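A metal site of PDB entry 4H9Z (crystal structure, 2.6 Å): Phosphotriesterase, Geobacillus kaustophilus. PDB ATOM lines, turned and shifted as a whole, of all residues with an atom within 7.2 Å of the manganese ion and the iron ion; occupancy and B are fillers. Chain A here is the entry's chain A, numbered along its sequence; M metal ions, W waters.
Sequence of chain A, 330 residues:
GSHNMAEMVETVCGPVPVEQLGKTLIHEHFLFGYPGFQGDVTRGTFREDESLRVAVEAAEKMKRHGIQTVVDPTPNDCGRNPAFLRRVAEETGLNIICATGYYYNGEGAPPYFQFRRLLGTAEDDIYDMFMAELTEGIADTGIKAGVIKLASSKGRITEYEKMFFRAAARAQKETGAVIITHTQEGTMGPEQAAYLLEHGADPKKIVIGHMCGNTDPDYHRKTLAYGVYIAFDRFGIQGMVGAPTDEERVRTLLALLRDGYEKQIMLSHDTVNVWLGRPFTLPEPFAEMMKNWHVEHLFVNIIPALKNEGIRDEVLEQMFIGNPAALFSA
Five residues have an atom within 4 Å of the manganese ion: Tyr 103, KCX 149, His 182, His 210 and Asp 270.
The manganese ion is bound by NE2 of His 210, OQ2 of KCX 149 and ND1 of His 182. Slightly farther from the manganese ion lies OH of Tyr 103 (2.9 Å).
OE1 of Gln 184 is in hydrogen-bond range of NE2 of His 182. A ring nitrogen (ND1) of His 27 sits at hydrogen-bond distance from the side-chain carboxylate (OD2) of Asp 233. The backbone NH of His 29 sits at hydrogen-bond distance from the backbone carbonyl oxygen of Thr 271 (2.6 Å). The guanidinium group (NE) of Arg 234 is in salt-bridge range of the side-chain carboxylate (OD2) of Asp 270, 3.7 Å away. The backbone NH (N) of His 182 lies within hydrogen-bond range of the backbone carbonyl oxygen (O) of Leu 150. ND1 of His 182 lies close to OH of Tyr 103. A ring nitrogen (ND1) of His 29 sits at hydrogen-bond distance from the side-chain hydroxyl (OG1) of Thr 74 (2.4 Å). The backbone carbonyl oxygen (O) of His 210 is in hydrogen-bond range of the side-chain hydroxyl (OG1) of Thr 183 (3.1 Å).
Of the 23 residues printed, 4 come within 4 Å of the iron ion. The nearest printed residue that does not touch the iron ion is His 210 (4.4 Å).
A ring nitrogen (NE2) of His 29 is bound to the iron ion (2.3 Å). NE2 of His 27 is bound to the iron ion, 2.4 Å away. The iron ion is bound by OD1 of Asp 270 (2.5 Å). The iron ion is bound by OQ1 of KCX 149.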
ATOM      1  N   HIS A  27      -4.035  18.214  24.127  1.00  0.00           N
ATOM      2  CA  HIS A  27      -4.909  19.327  24.476  1.00  0.00           C
ATOM      3  C   HIS A  27      -4.854  19.726  25.935  1.00  0.00           C
ATOM      4  O   HIS A  27      -5.628  19.223  26.738  1.00  0.00           O
ATOM      5  CB  HIS A  27      -6.359  18.950  24.130  1.00  0.00           C
ATOM      6  CG  HIS A  27      -7.239  20.129  23.894  1.00  0.00           C
ATOM      7  ND1 HIS A  27      -8.038  20.247  22.769  1.00  0.00           N
ATOM      8  CD2 HIS A  27      -7.465  21.244  24.621  1.00  0.00           C
ATOM      9  CE1 HIS A  27      -8.706  21.378  22.829  1.00  0.00           C
ATOM     10  NE2 HIS A  27      -8.368  22.004  23.942  1.00  0.00           N
ATOM     11  N   GLU A  28      -3.955  20.650  26.270  1.00  0.00           N
ATOM     12  CA  GLU A  28      -3.896  21.227  27.619  1.00  0.00           C
ATOM     13  C   GLU A  28      -3.588  22.729  27.544  1.00  0.00           C
ATOM     14  O   GLU A  28      -2.794  23.151  26.693  1.00  0.00           O
ATOM     15  CB  GLU A  28      -2.794  20.567  28.447  1.00  0.00           C
ATOM     16  CG  GLU A  28      -2.707  19.047  28.383  1.00  0.00           C
ATOM     17  CD  GLU A  28      -3.836  18.351  29.096  1.00  0.00           C
ATOM     18  OE1 GLU A  28      -4.327  18.868  30.130  1.00  0.00           O
ATOM     19  OE2 GLU A  28      -4.238  17.271  28.613  1.00  0.00           O
ATOM     20  N   HIS A  29      -4.190  23.538  28.415  1.00  0.00           N
ATOM     21  CA  HIS A  29      -3.836  24.969  28.462  1.00  0.00           C
ATOM     22  C   HIS A  29      -2.963  25.329  29.677  1.00  0.00           C
ATOM     23  O   HIS A  29      -3.288  24.982  30.804  1.00  0.00           O
ATOM     24  CB  HIS A  29      -5.077  25.868  28.445  1.00  0.00           C
ATOM     25  CG  HIS A  29      -6.026  25.569  27.329  1.00  0.00           C
ATOM     26  ND1 HIS A  29      -5.976  26.230  26.118  1.00  0.00           N
ATOM     27  CD2 HIS A  29      -7.051  24.695  27.245  1.00  0.00           C
ATOM     28  CE1 HIS A  29      -6.933  25.772  25.330  1.00  0.00           C
ATOM     29  NE2 HIS A  29      -7.602  24.835  25.995  1.00  0.00           N
ATOM     30  N   PHE A  32      -5.206  30.343  30.142  1.00  0.00           N
ATOM     31  CA  PHE A  32      -6.497  30.508  29.496  1.00  0.00           C
ATOM     32  C   PHE A  32      -7.397  31.541  30.190  1.00  0.00           C
ATOM     33  O   PHE A  32      -7.464  31.634  31.419  1.00  0.00           O
ATOM     34  CB  PHE A  32      -7.228  29.171  29.334  1.00  0.00           C
ATOM     35  CG  PHE A  32      -8.549  29.285  28.617  1.00  0.00           C
ATOM     36  CD1 PHE A  32      -9.720  29.572  29.325  1.00  0.00           C
ATOM     37  CD2 PHE A  32      -8.635  29.098  27.255  1.00  0.00           C
ATOM     38  CE1 PHE A  32     -10.928  29.652  28.667  1.00  0.00           C
ATOM     39  CE2 PHE A  32      -9.843  29.178  26.597  1.00  0.00           C
ATOM     40  CZ  PHE A  32     -10.994  29.460  27.300  1.00  0.00           C
ATOM     41  N   PRO A  73      -3.573  24.530  22.518  1.00  0.00           N
ATOM     42  CA  PRO A  73      -4.499  25.093  21.515  1.00  0.00           C
ATOM     43  C   PRO A  73      -5.262  26.340  22.007  1.00  0.00           C
ATOM     44  O   PRO A  73      -6.358  26.581  21.556  1.00  0.00           O
ATOM     45  CB  PRO A  73      -5.493  23.964  21.336  1.00  0.00           C
ATOM     46  CG  PRO A  73      -5.595  23.375  22.733  1.00  0.00           C
ATOM     47  CD  PRO A  73      -4.250  23.555  23.391  1.00  0.00           C
ATOM     48  N   THR A  74      -4.678  27.099  22.920  1.00  0.00           N
ATOM     49  CA  THR A  74      -5.338  28.284  23.459  1.00  0.00           C
ATOM     50  C   THR A  74      -5.539  29.274  22.326  1.00  0.00           C
ATOM     51  O   THR A  74      -4.583  29.701  21.689  1.00  0.00           O
ATOM     52  CB  THR A  74      -4.496  28.919  24.587  1.00  0.00           C
ATOM     53  OG1 THR A  74      -4.367  27.991  25.671  1.00  0.00           O
ATOM     54  CG2 THR A  74      -5.117  30.179  25.084  1.00  0.00           C
ATOM     55  N   PRO A  75      -6.799  29.631  22.039  1.00  0.00           N
ATOM     56  CA  PRO A  75      -7.050  30.491  20.872  1.00  0.00           C
ATOM     57  C   PRO A  75      -6.482  31.896  21.075  1.00  0.00           C
ATOM     58  O   PRO A  75      -6.141  32.261  22.195  1.00  0.00           O
ATOM     59  CB  PRO A  75      -8.572  30.521  20.773  1.00  0.00           C
ATOM     60  CG  PRO A  75      -9.050  29.382  21.585  1.00  0.00           C
ATOM     61  CD  PRO A  75      -8.043  29.194  22.679  1.00  0.00           C
ATOM     62  N   TYR A 103     -11.940  31.397  19.210  1.00  0.00           N
ATOM     63  CA  TYR A 103     -12.987  30.574  19.737  1.00  0.00           C
ATOM     64  C   TYR A 103     -14.279  30.668  18.947  1.00  0.00           C
ATOM     65  O   TYR A 103     -14.402  31.432  17.998  1.00  0.00           O
ATOM     66  CB  TYR A 103     -13.230  30.891  21.188  1.00  0.00           C
ATOM     67  CG  TYR A 103     -13.260  29.679  22.037  1.00  0.00           C
ATOM     68  CD1 TYR A 103     -13.258  28.418  21.483  1.00  0.00           C
ATOM     69  CD2 TYR A 103     -13.288  29.790  23.402  1.00  0.00           C
ATOM     70  CE1 TYR A 103     -13.278  27.301  22.283  1.00  0.00           C
ATOM     71  CE2 TYR A 103     -13.299  28.678  24.192  1.00  0.00           C
ATOM     72  CZ  TYR A 103     -13.295  27.450  23.614  1.00  0.00           C
ATOM     73  OH  TYR A 103     -13.300  26.403  24.408  1.00  0.00           O
ATOM     74  N   TYR A 104     -15.205  29.795  19.290  1.00  0.00           N
ATOM     75  CA  TYR A 104     -16.532  29.727  18.719  1.00  0.00           C
ATOM     76  C   TYR A 104     -17.416  30.785  19.328  1.00  0.00           C
ATOM     77  O   TYR A 104     -17.101  31.309  20.363  1.00  0.00           O
ATOM     78  CB  TYR A 104     -17.144  28.330  18.915  1.00  0.00           C
ATOM     79  CG  TYR A 104     -17.617  28.067  20.298  1.00  0.00           C
ATOM     80  CD1 TYR A 104     -16.732  27.915  21.335  1.00  0.00           C
ATOM     81  CD2 TYR A 104     -18.943  28.030  20.574  1.00  0.00           C
ATOM     82  CE1 TYR A 104     -17.177  27.709  22.607  1.00  0.00           C
ATOM     83  CE2 TYR A 104     -19.398  27.802  21.827  1.00  0.00           C
ATOM     84  CZ  TYR A 104     -18.514  27.640  22.828  1.00  0.00           C
ATOM     85  OH  TYR A 104     -19.021  27.450  24.050  1.00  0.00           O
ATOM     86  N   GLU A 107     -18.432  31.224  23.407  1.00  0.00           N
ATOM     87  CA  GLU A 107     -17.370  31.616  24.293  1.00  0.00           C
ATOM     88  C   GLU A 107     -16.159  32.264  23.575  1.00  0.00           C
ATOM     89  O   GLU A 107     -15.080  32.316  24.102  1.00  0.00           O
ATOM     90  CB  GLU A 107     -16.993  30.469  25.224  1.00  0.00           C
ATOM     91  CG  GLU A 107     -18.105  30.111  26.185  1.00  0.00           C
ATOM     92  CD  GLU A 107     -17.733  29.074  27.202  1.00  0.00           C
ATOM     93  OE1 GLU A 107     -17.215  28.027  26.806  1.00  0.00           O
ATOM     94  OE2 GLU A 107     -17.954  29.306  28.401  1.00  0.00           O
ATOM     95  N   KCX A 149      -6.496  26.109  15.316  1.00  0.00           N
ATOM     96  CA  KCX A 149      -7.627  25.819  16.178  1.00  0.00           C
ATOM     97  CB  KCX A 149      -7.468  26.492  17.542  1.00  0.00           C
ATOM     98  CG  KCX A 149      -8.623  26.190  18.528  1.00  0.00           C
ATOM     99  CD  KCX A 149      -8.662  24.698  18.817  1.00  0.00           C
ATOM    100  CE  KCX A 149      -9.544  24.340  20.011  1.00  0.00           C
ATOM    101  NZ  KCX A 149      -9.018  24.946  21.258  1.00  0.00           N
ATOM    102  C   KCX A 149      -8.937  26.271  15.521  1.00  0.00           C
ATOM    103  O   KCX A 149      -9.062  27.410  15.043  1.00  0.00           O
ATOM    104  CX  KCX A 149      -9.862  24.934  22.278  1.00  0.00           C
ATOM    105  OQ1 KCX A 149      -9.567  25.438  23.377  1.00  0.00           O
ATOM    106  OQ2 KCX A 149     -10.960  24.400  22.085  1.00  0.00           O
ATOM    107  N   LEU A 150      -9.902  25.353  15.503  1.00  0.00           N
ATOM    108  CA  LEU A 150     -11.237  25.620  15.004  1.00  0.00           C
ATOM    109  C   LEU A 150     -12.273  25.254  16.062  1.00  0.00           C
ATOM    110  O   LEU A 150     -12.065  24.325  16.833  1.00  0.00           O
ATOM    111  CB  LEU A 150     -11.502  24.790  13.746  1.00  0.00           C
ATOM    112  CG  LEU A 150     -10.817  25.196  12.442  1.00  0.00           C
ATOM    113  CD1 LEU A 150     -11.468  24.452  11.290  1.00  0.00           C
ATOM    114  CD2 LEU A 150     -10.869  26.703  12.197  1.00  0.00           C
ATOM    115  N   ALA A 151     -13.383  25.977  16.098  1.00  0.00           N
ATOM    116  CA  ALA A 151     -14.494  25.643  16.999  1.00  0.00           C
ATOM    117  C   ALA A 151     -15.904  25.844  16.391  1.00  0.00           C
ATOM    118  O   ALA A 151     -16.131  26.761  15.596  1.00  0.00           O
ATOM    119  CB  ALA A 151     -14.360  26.393  18.272  1.00  0.00           C
ATOM    120  N   THR A 181      -9.697  20.829  16.597  1.00  0.00           N
ATOM    121  CA  THR A 181     -10.997  21.463  16.721  1.00  0.00           C
ATOM    122  C   THR A 181     -11.639  21.294  18.101  1.00  0.00           C
ATOM    123  O   THR A 181     -11.228  20.456  18.919  1.00  0.00           O
ATOM    124  CB  THR A 181     -12.005  20.916  15.693  1.00  0.00           C
ATOM    125  OG1 THR A 181     -12.475  19.640  16.126  1.00  0.00           O
ATOM    126  CG2 THR A 181     -11.370  20.789  14.316  1.00  0.00           C
ATOM    127  N   HIS A 182     -12.655  22.102  18.344  1.00  0.00           N
ATOM    128  CA  HIS A 182     -13.458  22.062  19.551  1.00  0.00           C
ATOM    129  C   HIS A 182     -14.876  21.722  19.129  1.00  0.00           C
ATOM    130  O   HIS A 182     -15.402  22.335  18.195  1.00  0.00           O
ATOM    131  CB  HIS A 182     -13.426  23.435  20.217  1.00  0.00           C
ATOM    132  CG  HIS A 182     -14.604  23.730  21.095  1.00  0.00           C
ATOM    133  ND1 HIS A 182     -14.501  23.799  22.470  1.00  0.00           N
ATOM    134  CD2 HIS A 182     -15.895  24.013  20.796  1.00  0.00           C
ATOM    135  CE1 HIS A 182     -15.688  24.101  22.977  1.00  0.00           C
ATOM    136  NE2 HIS A 182     -16.555  24.224  21.994  1.00  0.00           N
ATOM    137  N   THR A 183     -15.484  20.742  19.779  1.00  0.00           N
ATOM    138  CA  THR A 183     -16.910  20.515  19.553  1.00  0.00           C
ATOM    139  C   THR A 183     -17.640  20.900  20.816  1.00  0.00           C
ATOM    140  O   THR A 183     -17.128  20.741  21.930  1.00  0.00           O
ATOM    141  CB  THR A 183     -17.252  19.059  19.161  1.00  0.00           C
ATOM    142  OG1 THR A 183     -16.830  18.158  20.204  1.00  0.00           O
ATOM    143  CG2 THR A 183     -16.603  18.665  17.840  1.00  0.00           C
ATOM    144  N   GLN A 184     -18.841  21.441  20.625  1.00  0.00           N
ATOM    145  CA  GLN A 184     -19.617  21.904  21.758  1.00  0.00           C
ATOM    146  C   GLN A 184     -20.634  20.839  22.174  1.00  0.00           C
ATOM    147  O   GLN A 184     -21.502  20.442  21.383  1.00  0.00           O
ATOM    148  CB  GLN A 184     -20.312  23.216  21.417  1.00  0.00           C
ATOM    149  CG  GLN A 184     -20.997  23.867  22.609  1.00  0.00           C
ATOM    150  CD  GLN A 184     -20.025  24.249  23.731  1.00  0.00           C
ATOM    151  OE1 GLN A 184     -18.804  24.274  23.556  1.00  0.00           O
ATOM    152  NE2 GLN A 184     -20.580  24.543  24.892  1.00  0.00           N
ATOM    153  N   HIS A 210     -13.027  17.108  21.768  1.00  0.00           N
ATOM    154  CA  HIS A 210     -14.155  17.027  22.696  1.00  0.00           C
ATOM    155  C   HIS A 210     -15.150  15.958  22.288  1.00  0.00           C
ATOM    156  O   HIS A 210     -16.369  16.118  22.508  1.00  0.00           O
ATOM    157  CB  HIS A 210     -14.855  18.372  22.802  1.00  0.00           C
ATOM    158  CG  HIS A 210     -13.952  19.491  23.218  1.00  0.00           C
ATOM    159  ND1 HIS A 210     -12.708  19.277  23.769  1.00  0.00           N
ATOM    160  CD2 HIS A 210     -14.113  20.828  23.161  1.00  0.00           C
ATOM    161  CE1 HIS A 210     -12.142  20.433  24.031  1.00  0.00           C
ATOM    162  NE2 HIS A 210     -12.971  21.394  23.663  1.00  0.00           N
ATOM    163  N   ASP A 233     -10.467  14.544  25.022  1.00  0.00           N
ATOM    164  CA  ASP A 233      -9.477  15.472  25.545  1.00  0.00           C
ATOM    165  C   ASP A 233      -9.974  16.209  26.765  1.00  0.00           C
ATOM    166  O   ASP A 233      -9.390  17.213  27.159  1.00  0.00           O
ATOM    167  CB  ASP A 233      -9.044  16.459  24.450  1.00  0.00           C
ATOM    168  CG  ASP A 233     -10.222  17.093  23.724  1.00  0.00           C
ATOM    169  OD1 ASP A 233     -11.296  17.263  24.337  1.00  0.00           O
ATOM    170  OD2 ASP A 233     -10.076  17.422  22.534  1.00  0.00           O
ATOM    171  N   ARG A 234     -11.055  15.717  27.349  1.00  0.00           N
ATOM    172  CA  ARG A 234     -11.653  16.396  28.480  1.00  0.00           C
ATOM    173  C   ARG A 234     -11.756  15.518  29.726  1.00  0.00           C
ATOM    174  O   ARG A 234     -12.689  15.657  30.508  1.00  0.00           O
ATOM    175  CB  ARG A 234     -13.016  16.992  28.103  1.00  0.00           C
ATOM    176  CG  ARG A 234     -12.968  18.447  27.673  1.00  0.00           C
ATOM    177  CD  ARG A 234     -14.320  18.924  27.202  1.00  0.00           C
ATOM    178  NE  ARG A 234     -14.489  20.374  27.341  1.00  0.00           N
ATOM    179  CZ  ARG A 234     -15.531  21.058  26.854  1.00  0.00           C
ATOM    180  NH1 ARG A 234     -16.503  20.435  26.200  1.00  0.00           N
ATOM    181  NH2 ARG A 234     -15.587  22.377  27.019  1.00  0.00           N
ATOM    182  N   ASP A 270      -7.689  18.784  28.741  1.00  0.00           N
ATOM    183  CA  ASP A 270      -8.124  20.160  28.448  1.00  0.00           C
ATOM    184  C   ASP A 270      -7.987  21.045  29.694  1.00  0.00           C
ATOM    185  O   ASP A 270      -8.875  21.858  29.975  1.00  0.00           O
ATOM    186  CB  ASP A 270      -9.571  20.172  27.913  1.00  0.00           C
ATOM    187  CG  ASP A 270      -9.965  21.489  27.296  1.00  0.00           C
ATOM    188  OD1 ASP A 270      -9.158  22.442  27.406  1.00  0.00           O
ATOM    189  OD2 ASP A 270     -11.073  21.575  26.692  1.00  0.00           O
ATOM    190  N   THR A 271      -6.898  20.897  30.444  1.00  0.00           N
ATOM    191  CA  THR A 271      -6.747  21.676  31.675  1.00  0.00           C
ATOM    192  C   THR A 271      -6.440  23.121  31.360  1.00  0.00           C
ATOM    193  O   THR A 271      -6.026  23.465  30.253  1.00  0.00           O
ATOM    194  CB  THR A 271      -5.605  21.192  32.618  1.00  0.00           C
ATOM    195  OG1 THR A 271      -4.336  21.400  32.001  1.00  0.00           O
ATOM    196  CG2 THR A 271      -5.758  19.734  33.010  1.00  0.00           C
ATOM    197  N   VAL A 272      -6.679  23.953  32.384  1.00  0.00           N
ATOM    198  CA  VAL A 272      -6.268  25.343  32.446  1.00  0.00           C
ATOM    199  C   VAL A 272      -5.438  25.500  33.723  1.00  0.00           C
ATOM    200  O   VAL A 272      -5.974  25.619  34.832  1.00  0.00           O
ATOM    201  CB  VAL A 272      -7.479  26.299  32.493  1.00  0.00           C
ATOM    202  CG1 VAL A 272      -7.000  27.744  32.601  1.00  0.00           C
ATOM    203  CG2 VAL A 272      -8.331  26.116  31.275  1.00  0.00           C
HETATM  204 MN    MN M   1     -12.362  23.676  23.953  1.00  0.00          MN
HETATM  205 FE    FE M   2      -9.491  23.695  25.305  1.00  0.00          FE
HETATM  206  O   HOH W   1     -11.290  25.372  26.815  1.00  0.00           O
